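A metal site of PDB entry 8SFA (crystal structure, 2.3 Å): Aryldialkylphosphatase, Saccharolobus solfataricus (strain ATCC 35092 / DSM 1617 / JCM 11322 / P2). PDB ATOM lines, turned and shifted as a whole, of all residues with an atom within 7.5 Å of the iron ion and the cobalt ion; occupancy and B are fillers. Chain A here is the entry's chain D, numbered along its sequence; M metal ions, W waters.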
ATOM      1  N   HIS A  22       5.084  -7.558  15.683  1.00  0.00           N
ATOM      2  CA  HIS A  22       3.985  -7.419  16.653  1.00  0.00           C
ATOM      3  C   HIS A  22       3.966  -5.982  17.178  1.00  0.00           C
ATOM      4  O   HIS A  22       4.674  -5.655  18.141  1.00  0.00           O
ATOM      5  CB  HIS A  22       4.149  -8.433  17.795  1.00  0.00           C
ATOM      6  CG  HIS A  22       2.959  -8.538  18.708  1.00  0.00           C
ATOM      7  ND1 HIS A  22       2.457  -9.746  19.143  1.00  0.00           N
ATOM      8  CD2 HIS A  22       2.176  -7.592  19.287  1.00  0.00           C
ATOM      9  CE1 HIS A  22       1.417  -9.545  19.936  1.00  0.00           C
ATOM     10  NE2 HIS A  22       1.231  -8.243  20.041  1.00  0.00           N
ATOM     11  N   GLU A  23       3.138  -5.129  16.544  1.00  0.00           N
ATOM     12  CA  GLU A  23       2.929  -3.746  16.959  1.00  0.00           C
ATOM     13  C   GLU A  23       1.474  -3.339  16.689  1.00  0.00           C
ATOM     14  O   GLU A  23       0.860  -3.801  15.724  1.00  0.00           O
ATOM     15  CB  GLU A  23       3.851  -2.763  16.209  1.00  0.00           C
ATOM     16  CG  GLU A  23       5.316  -3.153  16.121  1.00  0.00           C
ATOM     17  CD  GLU A  23       6.088  -3.024  17.458  1.00  0.00           C
ATOM     18  OE1 GLU A  23       7.169  -3.649  17.517  1.00  0.00           O
ATOM     19  OE2 GLU A  23       5.640  -2.326  18.415  1.00  0.00           O
ATOM     20  N   HIS A  24       0.949  -2.429  17.527  1.00  0.00           N
ATOM     21  CA  HIS A  24      -0.457  -1.996  17.451  1.00  0.00           C
ATOM     22  C   HIS A  24      -0.584  -0.514  17.125  1.00  0.00           C
ATOM     23  O   HIS A  24      -0.150   0.347  17.898  1.00  0.00           O
ATOM     24  CB  HIS A  24      -1.192  -2.269  18.769  1.00  0.00           C
ATOM     25  CG  HIS A  24      -1.204  -3.708  19.173  1.00  0.00           C
ATOM     26  ND1 HIS A  24      -2.190  -4.575  18.785  1.00  0.00           N
ATOM     27  CD2 HIS A  24      -0.341  -4.420  19.932  1.00  0.00           C
ATOM     28  CE1 HIS A  24      -1.941  -5.771  19.301  1.00  0.00           C
ATOM     29  NE2 HIS A  24      -0.828  -5.704  19.995  1.00  0.00           N
ATOM     30  N   VAL A  27      -5.658   0.594  19.899  1.00  0.00           N
ATOM     31  CA  VAL A  27      -6.304  -0.456  20.685  1.00  0.00           C
ATOM     32  C   VAL A  27      -7.431   0.153  21.516  1.00  0.00           C
ATOM     33  O   VAL A  27      -7.219   1.110  22.263  1.00  0.00           O
ATOM     34  CB  VAL A  27      -5.279  -1.170  21.593  1.00  0.00           C
ATOM     35  CG1 VAL A  27      -5.963  -1.915  22.723  1.00  0.00           C
ATOM     36  CG2 VAL A  27      -4.409  -2.121  20.779  1.00  0.00           C
ATOM     37  N   ASP A  66       0.350  -6.201  12.440  1.00  0.00           N
ATOM     38  CA  ASP A  66      -0.506  -5.593  13.465  1.00  0.00           C
ATOM     39  C   ASP A  66      -1.606  -6.571  13.885  1.00  0.00           C
ATOM     40  O   ASP A  66      -2.662  -6.636  13.234  1.00  0.00           O
ATOM     41  CB  ASP A  66      -1.105  -4.295  12.941  1.00  0.00           C
ATOM     42  CG  ASP A  66      -2.000  -3.587  13.952  1.00  0.00           C
ATOM     43  OD1 ASP A  66      -2.410  -4.181  14.968  1.00  0.00           O
ATOM     44  OD2 ASP A  66      -2.288  -2.392  13.726  1.00  0.00           O
ATOM     45  N   PRO A  67      -1.432  -7.307  15.001  1.00  0.00           N
ATOM     46  CA  PRO A  67      -2.392  -8.340  15.425  1.00  0.00           C
ATOM     47  C   PRO A  67      -3.526  -7.816  16.305  1.00  0.00           C
ATOM     48  O   PRO A  67      -3.829  -8.391  17.354  1.00  0.00           O
ATOM     49  CB  PRO A  67      -1.512  -9.324  16.185  1.00  0.00           C
ATOM     50  CG  PRO A  67      -0.456  -8.415  16.833  1.00  0.00           C
ATOM     51  CD  PRO A  67      -0.227  -7.268  15.856  1.00  0.00           C
ATOM     52  N   THR A  68      -4.148  -6.708  15.892  1.00  0.00           N
ATOM     53  CA  THR A  68      -5.310  -6.152  16.571  1.00  0.00           C
ATOM     54  C   THR A  68      -6.550  -6.790  15.957  1.00  0.00           C
ATOM     55  O   THR A  68      -6.776  -6.664  14.751  1.00  0.00           O
ATOM     56  CB  THR A  68      -5.362  -4.618  16.402  1.00  0.00           C
ATOM     57  OG1 THR A  68      -4.145  -4.014  16.860  1.00  0.00           O
ATOM     58  CG2 THR A  68      -6.542  -4.035  17.152  1.00  0.00           C
ATOM     59  N   CYS A  72     -10.185  -5.875  20.526  1.00  0.00           N
ATOM     60  CA  CYS A  72      -9.199  -4.817  20.704  1.00  0.00           C
ATOM     61  C   CYS A  72      -9.346  -3.669  19.710  1.00  0.00           C
ATOM     62  O   CYS A  72      -8.457  -2.822  19.637  1.00  0.00           O
ATOM     63  CB  CYS A  72      -7.761  -5.376  20.624  1.00  0.00           C
ATOM     64  SG  CYS A  72      -7.380  -6.639  21.878  1.00  0.00           S
ATOM     65  N   PHE A  97      -9.859 -12.154  20.447  1.00  0.00           N
ATOM     66  CA  PHE A  97      -8.976 -11.897  21.593  1.00  0.00           C
ATOM     67  C   PHE A  97      -9.832 -11.960  22.850  1.00  0.00           C
ATOM     68  O   PHE A  97     -10.449 -10.959  23.227  1.00  0.00           O
ATOM     69  CB  PHE A  97      -8.299 -10.523  21.484  1.00  0.00           C
ATOM     70  CG  PHE A  97      -7.152 -10.322  22.445  1.00  0.00           C
ATOM     71  CD1 PHE A  97      -7.392 -10.036  23.794  1.00  0.00           C
ATOM     72  CD2 PHE A  97      -5.835 -10.448  22.010  1.00  0.00           C
ATOM     73  CE1 PHE A  97      -6.338  -9.859  24.679  1.00  0.00           C
ATOM     74  CE2 PHE A  97      -4.772 -10.262  22.883  1.00  0.00           C
ATOM     75  CZ  PHE A  97      -5.022  -9.967  24.222  1.00  0.00           C
ATOM     76  N   PHE A  99      -9.957 -13.723  27.052  1.00  0.00           N
ATOM     77  CA  PHE A  99      -9.289 -14.427  28.143  1.00  0.00           C
ATOM     78  C   PHE A  99     -10.188 -15.436  28.851  1.00  0.00           C
ATOM     79  O   PHE A  99      -9.665 -16.358  29.496  1.00  0.00           O
ATOM     80  CB  PHE A  99      -8.768 -13.451  29.208  1.00  0.00           C
ATOM     81  CG  PHE A  99      -7.628 -12.579  28.751  1.00  0.00           C
ATOM     82  CD1 PHE A  99      -6.927 -12.862  27.588  1.00  0.00           C
ATOM     83  CD2 PHE A  99      -7.236 -11.476  29.509  1.00  0.00           C
ATOM     84  CE1 PHE A  99      -5.865 -12.063  27.179  1.00  0.00           C
ATOM     85  CE2 PHE A  99      -6.172 -10.656  29.108  1.00  0.00           C
ATOM     86  CZ  PHE A  99      -5.492 -10.939  27.938  1.00  0.00           C
ATOM     87  N   KCX A 137      -4.965 -14.540  14.911  1.00  0.00           N
ATOM     88  CA  KCX A 137      -4.516 -14.112  16.217  1.00  0.00           C
ATOM     89  CB  KCX A 137      -4.475 -12.590  16.279  1.00  0.00           C
ATOM     90  CG  KCX A 137      -4.244 -12.017  17.645  1.00  0.00           C
ATOM     91  CD  KCX A 137      -2.903 -12.435  18.186  1.00  0.00           C
ATOM     92  CE  KCX A 137      -2.750 -11.976  19.605  1.00  0.00           C
ATOM     93  NZ  KCX A 137      -2.800 -10.489  19.683  1.00  0.00           N
ATOM     94  C   KCX A 137      -5.441 -14.681  17.306  1.00  0.00           C
ATOM     95  O   KCX A 137      -6.631 -14.484  17.259  1.00  0.00           O
ATOM     96  CX  KCX A 137      -2.055  -9.887  20.596  1.00  0.00           C
ATOM     97  OQ1 KCX A 137      -2.018  -8.650  20.724  1.00  0.00           O
ATOM     98  OQ2 KCX A 137      -1.368 -10.585  21.328  1.00  0.00           O
ATOM     99  N   ILE A 138      -4.878 -15.427  18.243  1.00  0.00           N
ATOM    100  CA  ILE A 138      -5.676 -16.023  19.306  1.00  0.00           C
ATOM    101  C   ILE A 138      -4.999 -15.712  20.620  1.00  0.00           C
ATOM    102  O   ILE A 138      -3.841 -15.258  20.644  1.00  0.00           O
ATOM    103  CB  ILE A 138      -5.838 -17.545  19.099  1.00  0.00           C
ATOM    104  CG1 ILE A 138      -4.497 -18.234  19.309  1.00  0.00           C
ATOM    105  CG2 ILE A 138      -6.406 -17.867  17.699  1.00  0.00           C
ATOM    106  CD1 ILE A 138      -4.511 -19.691  18.984  1.00  0.00           C
ATOM    107  N   ALA A 139      -5.682 -15.986  21.738  1.00  0.00           N
ATOM    108  CA  ALA A 139      -5.156 -15.513  23.009  1.00  0.00           C
ATOM    109  C   ALA A 139      -5.563 -16.437  24.155  1.00  0.00           C
ATOM    110  O   ALA A 139      -6.602 -17.109  24.113  1.00  0.00           O
ATOM    111  CB  ALA A 139      -5.619 -14.081  23.325  1.00  0.00           C
ATOM    112  N   ASP A 141      -4.599 -16.173  28.718  1.00  0.00           N
ATOM    113  CA  ASP A 141      -3.796 -15.483  29.727  1.00  0.00           C
ATOM    114  C   ASP A 141      -3.941 -16.166  31.076  1.00  0.00           C
ATOM    115  O   ASP A 141      -4.102 -17.391  31.138  1.00  0.00           O
ATOM    116  CB  ASP A 141      -4.191 -14.006  29.795  1.00  0.00           C
ATOM    117  CG  ASP A 141      -3.027 -13.102  30.215  1.00  0.00           C
ATOM    118  OD1 ASP A 141      -2.139 -12.808  29.389  1.00  0.00           O
ATOM    119  OD2 ASP A 141      -2.980 -12.710  31.411  1.00  0.00           O
ATOM    120  N   THR A 169       0.024 -15.881  18.521  1.00  0.00           N
ATOM    121  CA  THR A 169      -0.730 -16.061  19.753  1.00  0.00           C
ATOM    122  C   THR A 169      -0.340 -15.022  20.801  1.00  0.00           C
ATOM    123  O   THR A 169       0.712 -14.362  20.720  1.00  0.00           O
ATOM    124  CB  THR A 169      -0.568 -17.466  20.371  1.00  0.00           C
ATOM    125  OG1 THR A 169       0.698 -17.546  21.055  1.00  0.00           O
ATOM    126  CG2 THR A 169      -0.632 -18.560  19.290  1.00  0.00           C
ATOM    127  N   HIS A 170      -1.239 -14.862  21.750  1.00  0.00           N
ATOM    128  CA  HIS A 170      -1.007 -14.149  23.002  1.00  0.00           C
ATOM    129  C   HIS A 170      -1.042 -15.190  24.104  1.00  0.00           C
ATOM    130  O   HIS A 170      -2.029 -15.928  24.232  1.00  0.00           O
ATOM    131  CB  HIS A 170      -2.077 -13.076  23.225  1.00  0.00           C
ATOM    132  CG  HIS A 170      -1.987 -12.392  24.552  1.00  0.00           C
ATOM    133  ND1 HIS A 170      -1.612 -11.066  24.684  1.00  0.00           N
ATOM    134  CD2 HIS A 170      -2.245 -12.839  25.806  1.00  0.00           C
ATOM    135  CE1 HIS A 170      -1.636 -10.734  25.966  1.00  0.00           C
ATOM    136  NE2 HIS A 170      -2.032 -11.781  26.665  1.00  0.00           N
ATOM    137  N   SER A 171       0.017 -15.264  24.889  1.00  0.00           N
ATOM    138  CA  SER A 171       0.041 -16.184  26.012  1.00  0.00           C
ATOM    139  C   SER A 171       0.622 -15.458  27.222  1.00  0.00           C
ATOM    140  O   SER A 171       1.175 -14.361  27.115  1.00  0.00           O
ATOM    141  CB  SER A 171       0.834 -17.449  25.683  1.00  0.00           C
ATOM    142  OG  SER A 171       2.191 -17.217  25.972  1.00  0.00           O
ATOM    143  N   GLY A 198       3.459 -16.141  21.511  1.00  0.00           N
ATOM    144  CA  GLY A 198       3.780 -14.790  21.892  1.00  0.00           C
ATOM    145  C   GLY A 198       4.014 -14.537  23.388  1.00  0.00           C
ATOM    146  O   GLY A 198       3.518 -15.262  24.265  1.00  0.00           O
ATOM    147  N   HIS A 199       4.781 -13.483  23.659  1.00  0.00           N
ATOM    148  CA  HIS A 199       5.046 -12.926  24.981  1.00  0.00           C
ATOM    149  C   HIS A 199       5.943 -13.822  25.832  1.00  0.00           C
ATOM    150  O   HIS A 199       5.982 -13.688  27.062  1.00  0.00           O
ATOM    151  CB  HIS A 199       3.717 -12.572  25.692  1.00  0.00           C
ATOM    152  CG  HIS A 199       2.848 -11.643  24.884  1.00  0.00           C
ATOM    153  ND1 HIS A 199       3.366 -10.707  24.015  1.00  0.00           N
ATOM    154  CD2 HIS A 199       1.498 -11.524  24.807  1.00  0.00           C
ATOM    155  CE1 HIS A 199       2.377 -10.043  23.452  1.00  0.00           C
ATOM    156  NE2 HIS A 199       1.228 -10.513  23.915  1.00  0.00           N
ATOM    157  N   ASP A 222       8.811 -10.314  22.281  1.00  0.00           N
ATOM    158  CA  ASP A 222       8.043  -9.333  21.526  1.00  0.00           C
ATOM    159  C   ASP A 222       7.459  -8.198  22.373  1.00  0.00           C
ATOM    160  O   ASP A 222       6.527  -7.525  21.922  1.00  0.00           O
ATOM    161  CB  ASP A 222       6.920 -10.059  20.770  1.00  0.00           C
ATOM    162  CG  ASP A 222       6.063 -10.916  21.712  1.00  0.00           C
ATOM    163  OD1 ASP A 222       6.027 -10.610  22.928  1.00  0.00           O
ATOM    164  OD2 ASP A 222       5.413 -11.883  21.233  1.00  0.00           O
ATOM    165  N   ARG A 223       7.986  -7.962  23.583  1.00  0.00           N
ATOM    166  CA  ARG A 223       7.460  -6.880  24.427  1.00  0.00           C
ATOM    167  C   ARG A 223       8.580  -5.984  24.965  1.00  0.00           C
ATOM    168  O   ARG A 223       8.521  -5.504  26.097  1.00  0.00           O
ATOM    169  CB  ARG A 223       6.614  -7.438  25.564  1.00  0.00           C
ATOM    170  CG  ARG A 223       5.124  -7.598  25.238  1.00  0.00           C
ATOM    171  CD  ARG A 223       4.288  -8.205  26.388  1.00  0.00           C
ATOM    172  NE  ARG A 223       2.851  -8.164  26.087  1.00  0.00           N
ATOM    173  CZ  ARG A 223       1.882  -8.693  26.844  1.00  0.00           C
ATOM    174  NH1 ARG A 223       0.599  -8.604  26.465  1.00  0.00           N
ATOM    175  NH2 ARG A 223       2.174  -9.331  27.973  1.00  0.00           N
ATOM    176  N   HIS A 255       7.979  -4.994  19.973  1.00  0.00           N
ATOM    177  CA  HIS A 255       7.734  -4.209  21.187  1.00  0.00           C
ATOM    178  C   HIS A 255       6.322  -4.289  21.736  1.00  0.00           C
ATOM    179  O   HIS A 255       6.131  -3.893  22.895  1.00  0.00           O
ATOM    180  CB  HIS A 255       8.035  -2.714  20.950  1.00  0.00           C
ATOM    181  CG  HIS A 255       9.347  -2.440  20.277  1.00  0.00           C
ATOM    182  ND1 HIS A 255       9.478  -2.402  18.905  1.00  0.00           N
ATOM    183  CD2 HIS A 255      10.566  -2.182  20.796  1.00  0.00           C
ATOM    184  CE1 HIS A 255      10.733  -2.132  18.607  1.00  0.00           C
ATOM    185  NE2 HIS A 255      11.414  -1.980  19.721  1.00  0.00           N
ATOM    186  N   ASP A 256       5.331  -4.759  20.969  1.00  0.00           N
ATOM    187  CA  ASP A 256       3.924  -4.723  21.374  1.00  0.00           C
ATOM    188  C   ASP A 256       3.469  -3.302  21.680  1.00  0.00           C
ATOM    189  O   ASP A 256       2.609  -3.063  22.525  1.00  0.00           O
ATOM    190  CB  ASP A 256       3.658  -5.645  22.590  1.00  0.00           C
ATOM    191  CG  ASP A 256       2.202  -6.139  22.685  1.00  0.00           C
ATOM    192  OD1 ASP A 256       1.419  -5.950  21.737  1.00  0.00           O
ATOM    193  OD2 ASP A 256       1.849  -6.731  23.742  1.00  0.00           O
ATOM    194  N   TYR A 257       4.038  -2.309  21.011  1.00  0.00           N
ATOM    195  CA  TYR A 257       3.671  -0.932  21.308  1.00  0.00           C
ATOM    196  C   TYR A 257       2.279  -0.601  20.792  1.00  0.00           C
ATOM    197  O   TYR A 257       1.806  -1.141  19.783  1.00  0.00           O
ATOM    198  CB  TYR A 257       4.706   0.023  20.727  1.00  0.00           C
ATOM    199  CG  TYR A 257       4.488   1.475  21.127  1.00  0.00           C
ATOM    200  CD1 TYR A 257       4.754   1.900  22.431  1.00  0.00           C
ATOM    201  CD2 TYR A 257       4.046   2.408  20.196  1.00  0.00           C
ATOM    202  CE1 TYR A 257       4.566   3.217  22.798  1.00  0.00           C
ATOM    203  CE2 TYR A 257       3.858   3.725  20.563  1.00  0.00           C
ATOM    204  CZ  TYR A 257       4.122   4.129  21.859  1.00  0.00           C
ATOM    205  OH  TYR A 257       3.912   5.446  22.219  1.00  0.00           O
ATOM    206  N   CYS A 258       1.595   0.294  21.513  1.00  0.00           N
ATOM    207  CA  CYS A 258       0.269   0.796  21.125  1.00  0.00           C
ATOM    208  C   CYS A 258       0.405   2.292  20.942  1.00  0.00           C
ATOM    209  O   CYS A 258       0.589   3.020  21.916  1.00  0.00           O
ATOM    210  CB  CYS A 258      -0.791   0.468  22.171  1.00  0.00           C
ATOM    211  SG  CYS A 258      -0.907  -1.281  22.658  1.00  0.00           S
HETATM  212 FE    FE M   1      -0.379  -7.226  21.180  1.00  0.00          FE
HETATM  213 CO    CO M   2      -0.716  -9.832  23.388  1.00  0.00          CO
HETATM  214  O   HOH W   1      -0.166  -7.958  23.426  1.00  0.00           O
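The iron ion is bound by NE2 of His 24 (2.0 Å), OQ1 of KCX 137 (2.2 Å), NE2 of His 22 (2.2 Å), OD1 of Asp 256 (2.3 Å) and water W1 (2.4 Å).
Arg 223 touches the cobalt ion (NH1 to CO, 3.6 Å).
Within 4 Å of the cobalt ion: KCX 137, His 170, His 199 and Arg 223.
Four residues have an atom within 4 Å of the iron ion: His 22, His 24, KCX 137 and Asp 256.
The nearest printed residue that does not touch the iron ion is Pro 67 (4.5 Å).
The backbone NH of His 24 sits at hydrogen-bond distance from the backbone carbonyl oxygen of Tyr 257 (2.7 Å).
N of His 170 is in hydrogen-bond range of O of Ile 138, at 2.9 Å.
A ring nitrogen (NE2) of His 170 is in hydrogen-bond range of the side-chain carboxylate (OD1) of Asp 141, 2.9 Å away.
A ring nitrogen (ND1) of His 199 lies close to the guanidinium group (NE) of Arg 223 (3.3 Å).
The side-chain carboxylate (OD1) of Asp 222 is in hydrogen-bond range of a ring nitrogen (ND1) of His 199 (2.9 Å).
NZ of KCX 137 sits at hydrogen-bond distance from O of Pro 67, at 3.3 Å.
OD2 of Asp 256 lies within salt-bridge range of NE of Arg 223 (2.9 Å).
The backbone NH (N) of Asp 256 lies within hydrogen-bond range of the backbone carbonyl oxygen (O) of Asp 222 (3.2 Å).
The cobalt ion is bound by water W1 (2.0 Å), a ring nitrogen (ND1) of His 170 (2.0 Å), a ring nitrogen (NE2) of His 199 (2.1 Å) and OQ2 of KCX 137 (2.3 Å).
The cobalt ion has four donor atoms within binding distance.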
